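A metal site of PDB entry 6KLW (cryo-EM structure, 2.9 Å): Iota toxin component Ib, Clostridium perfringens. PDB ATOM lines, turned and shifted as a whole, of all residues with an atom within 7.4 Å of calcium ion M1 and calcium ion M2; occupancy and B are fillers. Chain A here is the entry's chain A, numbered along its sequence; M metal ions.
Of the 25 residues printed, 5 come within 4 Å of calcium ion M2. The nearest printed residue that does not touch calcium ion M2 is Asp 18 (4.03 Å).
Calcium ion M1 is bound by the side-chain carboxylate (OD2) of Asp 12 (2.3 Å), the backbone carbonyl oxygen (O) of Glu 53 (2.3 Å), the backbone carbonyl oxygen (O) of Ser 50 (2.4 Å), the side-chain carboxylate (OE2) of Glu 21 (2.4 Å), the side-chain carboxylate (OD2) of Asp 63 (2.4 Å), the side-chain carboxylate (OD2) of Asp 14 (2.8 Å) and the side-chain carboxylate (OE1) of Glu 21 (2.9 Å).
Of the 25 residues printed, 6 come within 4 Å of calcium ion M1. Along chain A the residues within 4 Å of calcium ion M1 span positions 12 to 63. The nearest printed residue that does not touch calcium ion M1 is Tyr 51 (4.2 Å).
The side-chain hydroxyl (OG) of Ser 50 lies within hydrogen-bond range of the backbone NH (N) of Glu 53, 3.3 Å away. The backbone NH (N) of Ser 50 is in hydrogen-bond range of the side-chain hydroxyl (OG1) of Thr 56. N of Leu 52 sits close to OG of Ser 50, 3.4 Å away. O of Glu 21 sits at hydrogen-bond distance from N of Ser 49 (3.2 Å). The side-chain carboxylate (OD2) of Asp 10 is in hydrogen-bond range of the backbone NH (N) of Asn 15. The backbone carbonyl oxygen (O) of Ser 54 sits at hydrogen-bond distance from the backbone NH (N) of Asp 63. The side-chain hydroxyl (OG1) of Thr 56 sits at hydrogen-bond distance from the side-chain carboxylate (OD1) of Asp 63 (3.0 Å).
OD1 of Asp 12 is bound to calcium ion M2. Calcium ion M2 is bound by O of Ile 16, at 2.3 Å. The side-chain carboxylate (OD1) of Asp 10 is bound to calcium ion M2. OD1 of Asp 14 is bound to calcium ion M2, 2.5 Å away. Calcium ion M2 is bound by OE1 of Glu 21. Slightly farther from calcium ion M2 lies the side-chain carboxylate (OD2) of Asp 12 (3.0 Å).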
ATOM      1  N   LEU A   9     -19.853  30.455   6.533  1.00  0.00           N
ATOM      2  CA  LEU A   9     -19.337  30.938   5.257  1.00  0.00           C
ATOM      3  C   LEU A   9     -20.191  30.357   4.154  1.00  0.00           C
ATOM      4  O   LEU A   9     -20.273  29.137   3.995  1.00  0.00           O
ATOM      5  CB  LEU A   9     -17.873  30.529   5.063  1.00  0.00           C
ATOM      6  CG  LEU A   9     -17.147  31.109   3.857  1.00  0.00           C
ATOM      7  CD1 LEU A   9     -17.496  32.567   3.666  1.00  0.00           C
ATOM      8  CD2 LEU A   9     -15.651  30.939   4.014  1.00  0.00           C
ATOM      9  N   ASP A  10     -20.832  31.228   3.380  1.00  0.00           N
ATOM     10  CA  ASP A  10     -21.741  30.825   2.321  1.00  0.00           C
ATOM     11  C   ASP A  10     -21.259  31.494   1.038  1.00  0.00           C
ATOM     12  O   ASP A  10     -21.578  32.648   0.758  1.00  0.00           O
ATOM     13  CB  ASP A  10     -23.169  31.224   2.659  1.00  0.00           C
ATOM     14  CG  ASP A  10     -24.190  30.355   1.973  1.00  0.00           C
ATOM     15  OD1 ASP A  10     -23.805  29.348   1.348  1.00  0.00           O
ATOM     16  OD2 ASP A  10     -25.386  30.689   2.064  1.00  0.00           O
ATOM     17  N   THR A  11     -20.472  30.747   0.250  1.00  0.00           N
ATOM     18  CA  THR A  11     -19.955  31.297  -0.992  1.00  0.00           C
ATOM     19  C   THR A  11     -21.067  31.455  -2.029  1.00  0.00           C
ATOM     20  O   THR A  11     -21.204  32.515  -2.649  1.00  0.00           O
ATOM     21  CB  THR A  11     -18.835  30.416  -1.526  1.00  0.00           C
ATOM     22  OG1 THR A  11     -17.740  30.421  -0.610  1.00  0.00           O
ATOM     23  CG2 THR A  11     -18.353  30.945  -2.863  1.00  0.00           C
ATOM     24  N   ASP A  12     -21.869  30.413  -2.228  1.00  0.00           N
ATOM     25  CA  ASP A  12     -22.946  30.438  -3.205  1.00  0.00           C
ATOM     26  C   ASP A  12     -24.169  31.197  -2.707  1.00  0.00           C
ATOM     27  O   ASP A  12     -25.081  31.433  -3.511  1.00  0.00           O
ATOM     28  CB  ASP A  12     -23.356  29.017  -3.567  1.00  0.00           C
ATOM     29  CG  ASP A  12     -23.506  28.133  -2.366  1.00  0.00           C
ATOM     30  OD1 ASP A  12     -23.015  28.506  -1.293  1.00  0.00           O
ATOM     31  OD2 ASP A  12     -24.130  27.058  -2.485  1.00  0.00           O
ATOM     32  N   ASN A  13     -24.218  31.560  -1.432  1.00  0.00           N
ATOM     33  CA  ASN A  13     -25.294  32.358  -0.852  1.00  0.00           C
ATOM     34  C   ASN A  13     -26.648  31.666  -1.018  1.00  0.00           C
ATOM     35  O   ASN A  13     -27.637  32.269  -1.435  1.00  0.00           O
ATOM     36  CB  ASN A  13     -25.327  33.762  -1.468  1.00  0.00           C
ATOM     37  CG  ASN A  13     -24.216  34.641  -0.939  1.00  0.00           C
ATOM     38  OD1 ASN A  13     -23.299  35.008  -1.676  1.00  0.00           O
ATOM     39  ND2 ASN A  13     -24.288  34.985   0.333  1.00  0.00           N
ATOM     40  N   ASP A  14     -26.685  30.389  -0.648  1.00  0.00           N
ATOM     41  CA  ASP A  14     -27.909  29.606  -0.717  1.00  0.00           C
ATOM     42  C   ASP A  14     -28.369  29.156   0.660  1.00  0.00           C
ATOM     43  O   ASP A  14     -29.154  28.215   0.779  1.00  0.00           O
ATOM     44  CB  ASP A  14     -27.731  28.398  -1.642  1.00  0.00           C
ATOM     45  CG  ASP A  14     -26.703  27.427  -1.132  1.00  0.00           C
ATOM     46  OD1 ASP A  14     -25.843  27.826  -0.326  1.00  0.00           O
ATOM     47  OD2 ASP A  14     -26.750  26.255  -1.554  1.00  0.00           O
ATOM     48  N   ASN A  15     -27.866  29.812   1.707  1.00  0.00           N
ATOM     49  CA  ASN A  15     -28.250  29.627   3.101  1.00  0.00           C
ATOM     50  C   ASN A  15     -27.778  28.316   3.701  1.00  0.00           C
ATOM     51  O   ASN A  15     -28.384  27.823   4.651  1.00  0.00           O
ATOM     52  CB  ASN A  15     -29.776  29.724   3.289  1.00  0.00           C
ATOM     53  CG  ASN A  15     -30.289  31.110   3.053  1.00  0.00           C
ATOM     54  OD1 ASN A  15     -29.529  32.063   2.944  1.00  0.00           O
ATOM     55  ND2 ASN A  15     -31.618  31.232   2.965  1.00  0.00           N
ATOM     56  N   ILE A  16     -26.713  27.725   3.177  1.00  0.00           N
ATOM     57  CA  ILE A  16     -26.115  26.530   3.753  1.00  0.00           C
ATOM     58  C   ILE A  16     -24.603  26.759   3.796  1.00  0.00           C
ATOM     59  O   ILE A  16     -23.979  26.988   2.759  1.00  0.00           O
ATOM     60  CB  ILE A  16     -26.439  25.269   2.940  1.00  0.00           C
ATOM     61  CG1 ILE A  16     -27.940  25.112   2.761  1.00  0.00           C
ATOM     62  CG2 ILE A  16     -25.907  24.051   3.663  1.00  0.00           C
ATOM     63  CD1 ILE A  16     -28.324  24.082   1.739  1.00  0.00           C
ATOM     64  N   PRO A  17     -23.983  26.721   4.976  1.00  0.00           N
ATOM     65  CA  PRO A  17     -22.532  26.988   5.051  1.00  0.00           C
ATOM     66  C   PRO A  17     -21.724  25.969   4.266  1.00  0.00           C
ATOM     67  O   PRO A  17     -22.194  24.877   3.938  1.00  0.00           O
ATOM     68  CB  PRO A  17     -22.250  26.900   6.552  1.00  0.00           C
ATOM     69  CG  PRO A  17     -23.541  27.234   7.194  1.00  0.00           C
ATOM     70  CD  PRO A  17     -24.596  26.664   6.304  1.00  0.00           C
ATOM     71  N   ASP A  18     -20.486  26.342   3.966  1.00  0.00           N
ATOM     72  CA  ASP A  18     -19.624  25.540   3.107  1.00  0.00           C
ATOM     73  C   ASP A  18     -19.277  24.200   3.733  1.00  0.00           C
ATOM     74  O   ASP A  18     -19.261  23.167   3.054  1.00  0.00           O
ATOM     75  CB  ASP A  18     -18.355  26.307   2.773  1.00  0.00           C
ATOM     76  CG  ASP A  18     -18.611  27.502   1.895  1.00  0.00           C
ATOM     77  OD1 ASP A  18     -19.786  27.733   1.546  1.00  0.00           O
ATOM     78  OD2 ASP A  18     -17.648  28.215   1.555  1.00  0.00           O
ATOM     79  N   ALA A  19     -18.973  24.202   5.035  1.00  0.00           N
ATOM     80  CA  ALA A  19     -18.649  22.954   5.722  1.00  0.00           C
ATOM     81  C   ALA A  19     -19.813  21.982   5.671  1.00  0.00           C
ATOM     82  O   ALA A  19     -19.605  20.778   5.469  1.00  0.00           O
ATOM     83  CB  ALA A  19     -18.250  23.238   7.159  1.00  0.00           C
ATOM     84  N   GLU A  21     -22.194  21.764   3.433  1.00  0.00           N
ATOM     85  CA  GLU A  21     -22.386  21.220   2.093  1.00  0.00           C
ATOM     86  C   GLU A  21     -21.275  20.260   1.684  1.00  0.00           C
ATOM     87  O   GLU A  21     -21.546  19.275   0.995  1.00  0.00           O
ATOM     88  CB  GLU A  21     -22.519  22.339   1.074  1.00  0.00           C
ATOM     89  CG  GLU A  21     -23.919  22.884   0.988  1.00  0.00           C
ATOM     90  CD  GLU A  21     -24.041  24.036   0.048  1.00  0.00           C
ATOM     91  OE1 GLU A  21     -23.003  24.627  -0.298  1.00  0.00           O
ATOM     92  OE2 GLU A  21     -25.165  24.350  -0.378  1.00  0.00           O
ATOM     93  N   TYR A  25     -25.400  17.354   5.961  1.00  0.00           N
ATOM     94  CA  TYR A  25     -26.255  18.281   6.689  1.00  0.00           C
ATOM     95  C   TYR A  25     -27.693  17.802   6.571  1.00  0.00           C
ATOM     96  O   TYR A  25     -27.988  16.828   5.867  1.00  0.00           O
ATOM     97  CB  TYR A  25     -26.131  19.716   6.164  1.00  0.00           C
ATOM     98  CG  TYR A  25     -26.633  19.954   4.756  1.00  0.00           C
ATOM     99  CD1 TYR A  25     -27.907  20.432   4.524  1.00  0.00           C
ATOM    100  CD2 TYR A  25     -25.819  19.706   3.670  1.00  0.00           C
ATOM    101  CE1 TYR A  25     -28.363  20.639   3.250  1.00  0.00           C
ATOM    102  CE2 TYR A  25     -26.264  19.918   2.387  1.00  0.00           C
ATOM    103  CZ  TYR A  25     -27.534  20.386   2.181  1.00  0.00           C
ATOM    104  OH  TYR A  25     -27.979  20.597   0.899  1.00  0.00           O
ATOM    105  N   SER A  49     -23.864  18.622  -1.148  1.00  0.00           N
ATOM    106  CA  SER A  49     -24.116  19.501  -2.267  1.00  0.00           C
ATOM    107  C   SER A  49     -22.796  20.099  -2.734  1.00  0.00           C
ATOM    108  O   SER A  49     -21.738  19.832  -2.165  1.00  0.00           O
ATOM    109  CB  SER A  49     -25.111  20.610  -1.891  1.00  0.00           C
ATOM    110  OG  SER A  49     -26.351  20.060  -1.503  1.00  0.00           O
ATOM    111  N   SER A  50     -22.870  20.904  -3.781  1.00  0.00           N
ATOM    112  CA  SER A  50     -21.723  21.688  -4.211  1.00  0.00           C
ATOM    113  C   SER A  50     -21.704  23.006  -3.462  1.00  0.00           C
ATOM    114  O   SER A  50     -22.667  23.778  -3.507  1.00  0.00           O
ATOM    115  CB  SER A  50     -21.778  21.933  -5.715  1.00  0.00           C
ATOM    116  OG  SER A  50     -20.851  22.922  -6.099  1.00  0.00           O
ATOM    117  N   TYR A  51     -20.612  23.283  -2.757  1.00  0.00           N
ATOM    118  CA  TYR A  51     -20.536  24.506  -1.977  1.00  0.00           C
ATOM    119  C   TYR A  51     -20.254  25.729  -2.829  1.00  0.00           C
ATOM    120  O   TYR A  51     -20.223  26.840  -2.297  1.00  0.00           O
ATOM    121  CB  TYR A  51     -19.496  24.365  -0.868  1.00  0.00           C
ATOM    122  CG  TYR A  51     -18.049  24.526  -1.291  1.00  0.00           C
ATOM    123  CD1 TYR A  51     -17.446  25.772  -1.280  1.00  0.00           C
ATOM    124  CD2 TYR A  51     -17.300  23.430  -1.674  1.00  0.00           C
ATOM    125  CE1 TYR A  51     -16.131  25.919  -1.654  1.00  0.00           C
ATOM    126  CE2 TYR A  51     -15.990  23.573  -2.057  1.00  0.00           C
ATOM    127  CZ  TYR A  51     -15.412  24.816  -2.043  1.00  0.00           C
ATOM    128  OH  TYR A  51     -14.097  24.963  -2.417  1.00  0.00           O
ATOM    129  N   LEU A  52     -20.083  25.572  -4.139  1.00  0.00           N
ATOM    130  CA  LEU A  52     -19.835  26.677  -5.045  1.00  0.00           C
ATOM    131  C   LEU A  52     -20.987  26.897  -6.021  1.00  0.00           C
ATOM    132  O   LEU A  52     -20.951  27.838  -6.807  1.00  0.00           O
ATOM    133  CB  LEU A  52     -18.537  26.452  -5.823  1.00  0.00           C
ATOM    134  CG  LEU A  52     -17.249  26.675  -5.026  1.00  0.00           C
ATOM    135  CD1 LEU A  52     -16.061  26.161  -5.779  1.00  0.00           C
ATOM    136  CD2 LEU A  52     -17.085  28.135  -4.708  1.00  0.00           C
ATOM    137  N   GLU A  53     -22.011  26.050  -5.973  1.00  0.00           N
ATOM    138  CA  GLU A  53     -23.207  26.186  -6.789  1.00  0.00           C
ATOM    139  C   GLU A  53     -24.417  26.314  -5.886  1.00  0.00           C
ATOM    140  O   GLU A  53     -24.494  25.658  -4.849  1.00  0.00           O
ATOM    141  CB  GLU A  53     -23.377  24.990  -7.734  1.00  0.00           C
ATOM    142  CG  GLU A  53     -22.536  25.060  -8.981  1.00  0.00           C
ATOM    143  CD  GLU A  53     -23.108  26.002 -10.023  1.00  0.00           C
ATOM    144  OE1 GLU A  53     -24.276  26.413  -9.870  1.00  0.00           O
ATOM    145  OE2 GLU A  53     -22.389  26.316 -10.991  1.00  0.00           O
ATOM    146  N   SER A  54     -25.363  27.159  -6.281  1.00  0.00           N
ATOM    147  CA  SER A  54     -26.607  27.263  -5.535  1.00  0.00           C
ATOM    148  C   SER A  54     -27.656  26.303  -6.067  1.00  0.00           C
ATOM    149  O   SER A  54     -28.577  25.915  -5.344  1.00  0.00           O
ATOM    150  CB  SER A  54     -27.122  28.697  -5.592  1.00  0.00           C
ATOM    151  OG  SER A  54     -27.515  29.030  -6.907  1.00  0.00           O
ATOM    152  N   ASN A  55     -27.526  25.901  -7.324  1.00  0.00           N
ATOM    153  CA  ASN A  55     -28.423  24.952  -7.977  1.00  0.00           C
ATOM    154  C   ASN A  55     -27.554  23.786  -8.453  1.00  0.00           C
ATOM    155  O   ASN A  55     -27.069  23.776  -9.578  1.00  0.00           O
ATOM    156  CB  ASN A  55     -29.152  25.583  -9.154  1.00  0.00           C
ATOM    157  CG  ASN A  55     -30.279  26.493  -8.714  1.00  0.00           C
ATOM    158  OD1 ASN A  55     -31.433  26.089  -8.662  1.00  0.00           O
ATOM    159  ND2 ASN A  55     -29.946  27.732  -8.454  1.00  0.00           N
ATOM    160  N   THR A  56     -27.363  22.805  -7.575  1.00  0.00           N
ATOM    161  CA  THR A  56     -26.391  21.746  -7.860  1.00  0.00           C
ATOM    162  C   THR A  56     -26.880  20.821  -8.964  1.00  0.00           C
ATOM    163  O   THR A  56     -26.123  20.449  -9.865  1.00  0.00           O
ATOM    164  CB  THR A  56     -26.088  20.967  -6.590  1.00  0.00           C
ATOM    165  OG1 THR A  56     -25.496  21.847  -5.628  1.00  0.00           O
ATOM    166  CG2 THR A  56     -25.147  19.824  -6.871  1.00  0.00           C
ATOM    167  N   THR A  62     -33.094  25.732  -5.693  1.00  0.00           N
ATOM    168  CA  THR A  62     -31.777  25.777  -5.075  1.00  0.00           C
ATOM    169  C   THR A  62     -31.597  24.624  -4.106  1.00  0.00           C
ATOM    170  O   THR A  62     -32.533  23.878  -3.806  1.00  0.00           O
ATOM    171  CB  THR A  62     -31.558  27.117  -4.367  1.00  0.00           C
ATOM    172  OG1 THR A  62     -32.432  27.202  -3.239  1.00  0.00           O
ATOM    173  CG2 THR A  62     -31.836  28.262  -5.298  1.00  0.00           C
ATOM    174  N   ASP A  63     -30.373  24.468  -3.608  1.00  0.00           N
ATOM    175  CA  ASP A  63     -30.077  23.395  -2.668  1.00  0.00           C
ATOM    176  C   ASP A  63     -30.947  23.499  -1.427  1.00  0.00           C
ATOM    177  O   ASP A  63     -31.472  22.490  -0.927  1.00  0.00           O
ATOM    178  CB  ASP A  63     -28.595  23.424  -2.290  1.00  0.00           C
ATOM    179  CG  ASP A  63     -27.695  23.072  -3.445  1.00  0.00           C
ATOM    180  OD1 ASP A  63     -28.108  22.273  -4.300  1.00  0.00           O
ATOM    181  OD2 ASP A  63     -26.562  23.592  -3.497  1.00  0.00           O
ATOM    182  N   TYR A  64     -31.128  24.715  -0.912  1.00  0.00           N
ATOM    183  CA  TYR A  64     -31.926  24.886   0.296  1.00  0.00           C
ATOM    184  C   TYR A  64     -33.409  24.646   0.030  1.00  0.00           C
ATOM    185  O   TYR A  64     -34.108  24.079   0.870  1.00  0.00           O
ATOM    186  CB  TYR A  64     -31.714  26.281   0.873  1.00  0.00           C
ATOM    187  CG  TYR A  64     -32.512  26.507   2.132  1.00  0.00           C
ATOM    188  CD1 TYR A  64     -32.111  25.975   3.340  1.00  0.00           C
ATOM    189  CD2 TYR A  64     -33.689  27.247   2.104  1.00  0.00           C
ATOM    190  CE1 TYR A  64     -32.833  26.172   4.492  1.00  0.00           C
ATOM    191  CE2 TYR A  64     -34.423  27.445   3.250  1.00  0.00           C
ATOM    192  CZ  TYR A  64     -33.985  26.911   4.436  1.00  0.00           C
ATOM    193  OH  TYR A  64     -34.719  27.109   5.582  1.00  0.00           O
ATOM    194  N   PRO A  82     -30.641  17.311  -3.055  1.00  0.00           N
ATOM    195  CA  PRO A  82     -29.987  18.273  -3.946  1.00  0.00           C
ATOM    196  C   PRO A  82     -29.271  17.652  -5.140  1.00  0.00           C
ATOM    197  O   PRO A  82     -28.890  18.393  -6.059  1.00  0.00           O
ATOM    198  CB  PRO A  82     -29.005  18.989  -3.012  1.00  0.00           C
ATOM    199  CG  PRO A  82     -29.654  18.915  -1.692  1.00  0.00           C
ATOM    200  CD  PRO A  82     -30.332  17.582  -1.646  1.00  0.00           C
HETATM  201 CA    CA M   1     -24.649  24.800  -2.667  1.00  0.00          CA
HETATM  202 CA    CA M   2     -23.617  27.122   0.447  1.00  0.00          CA
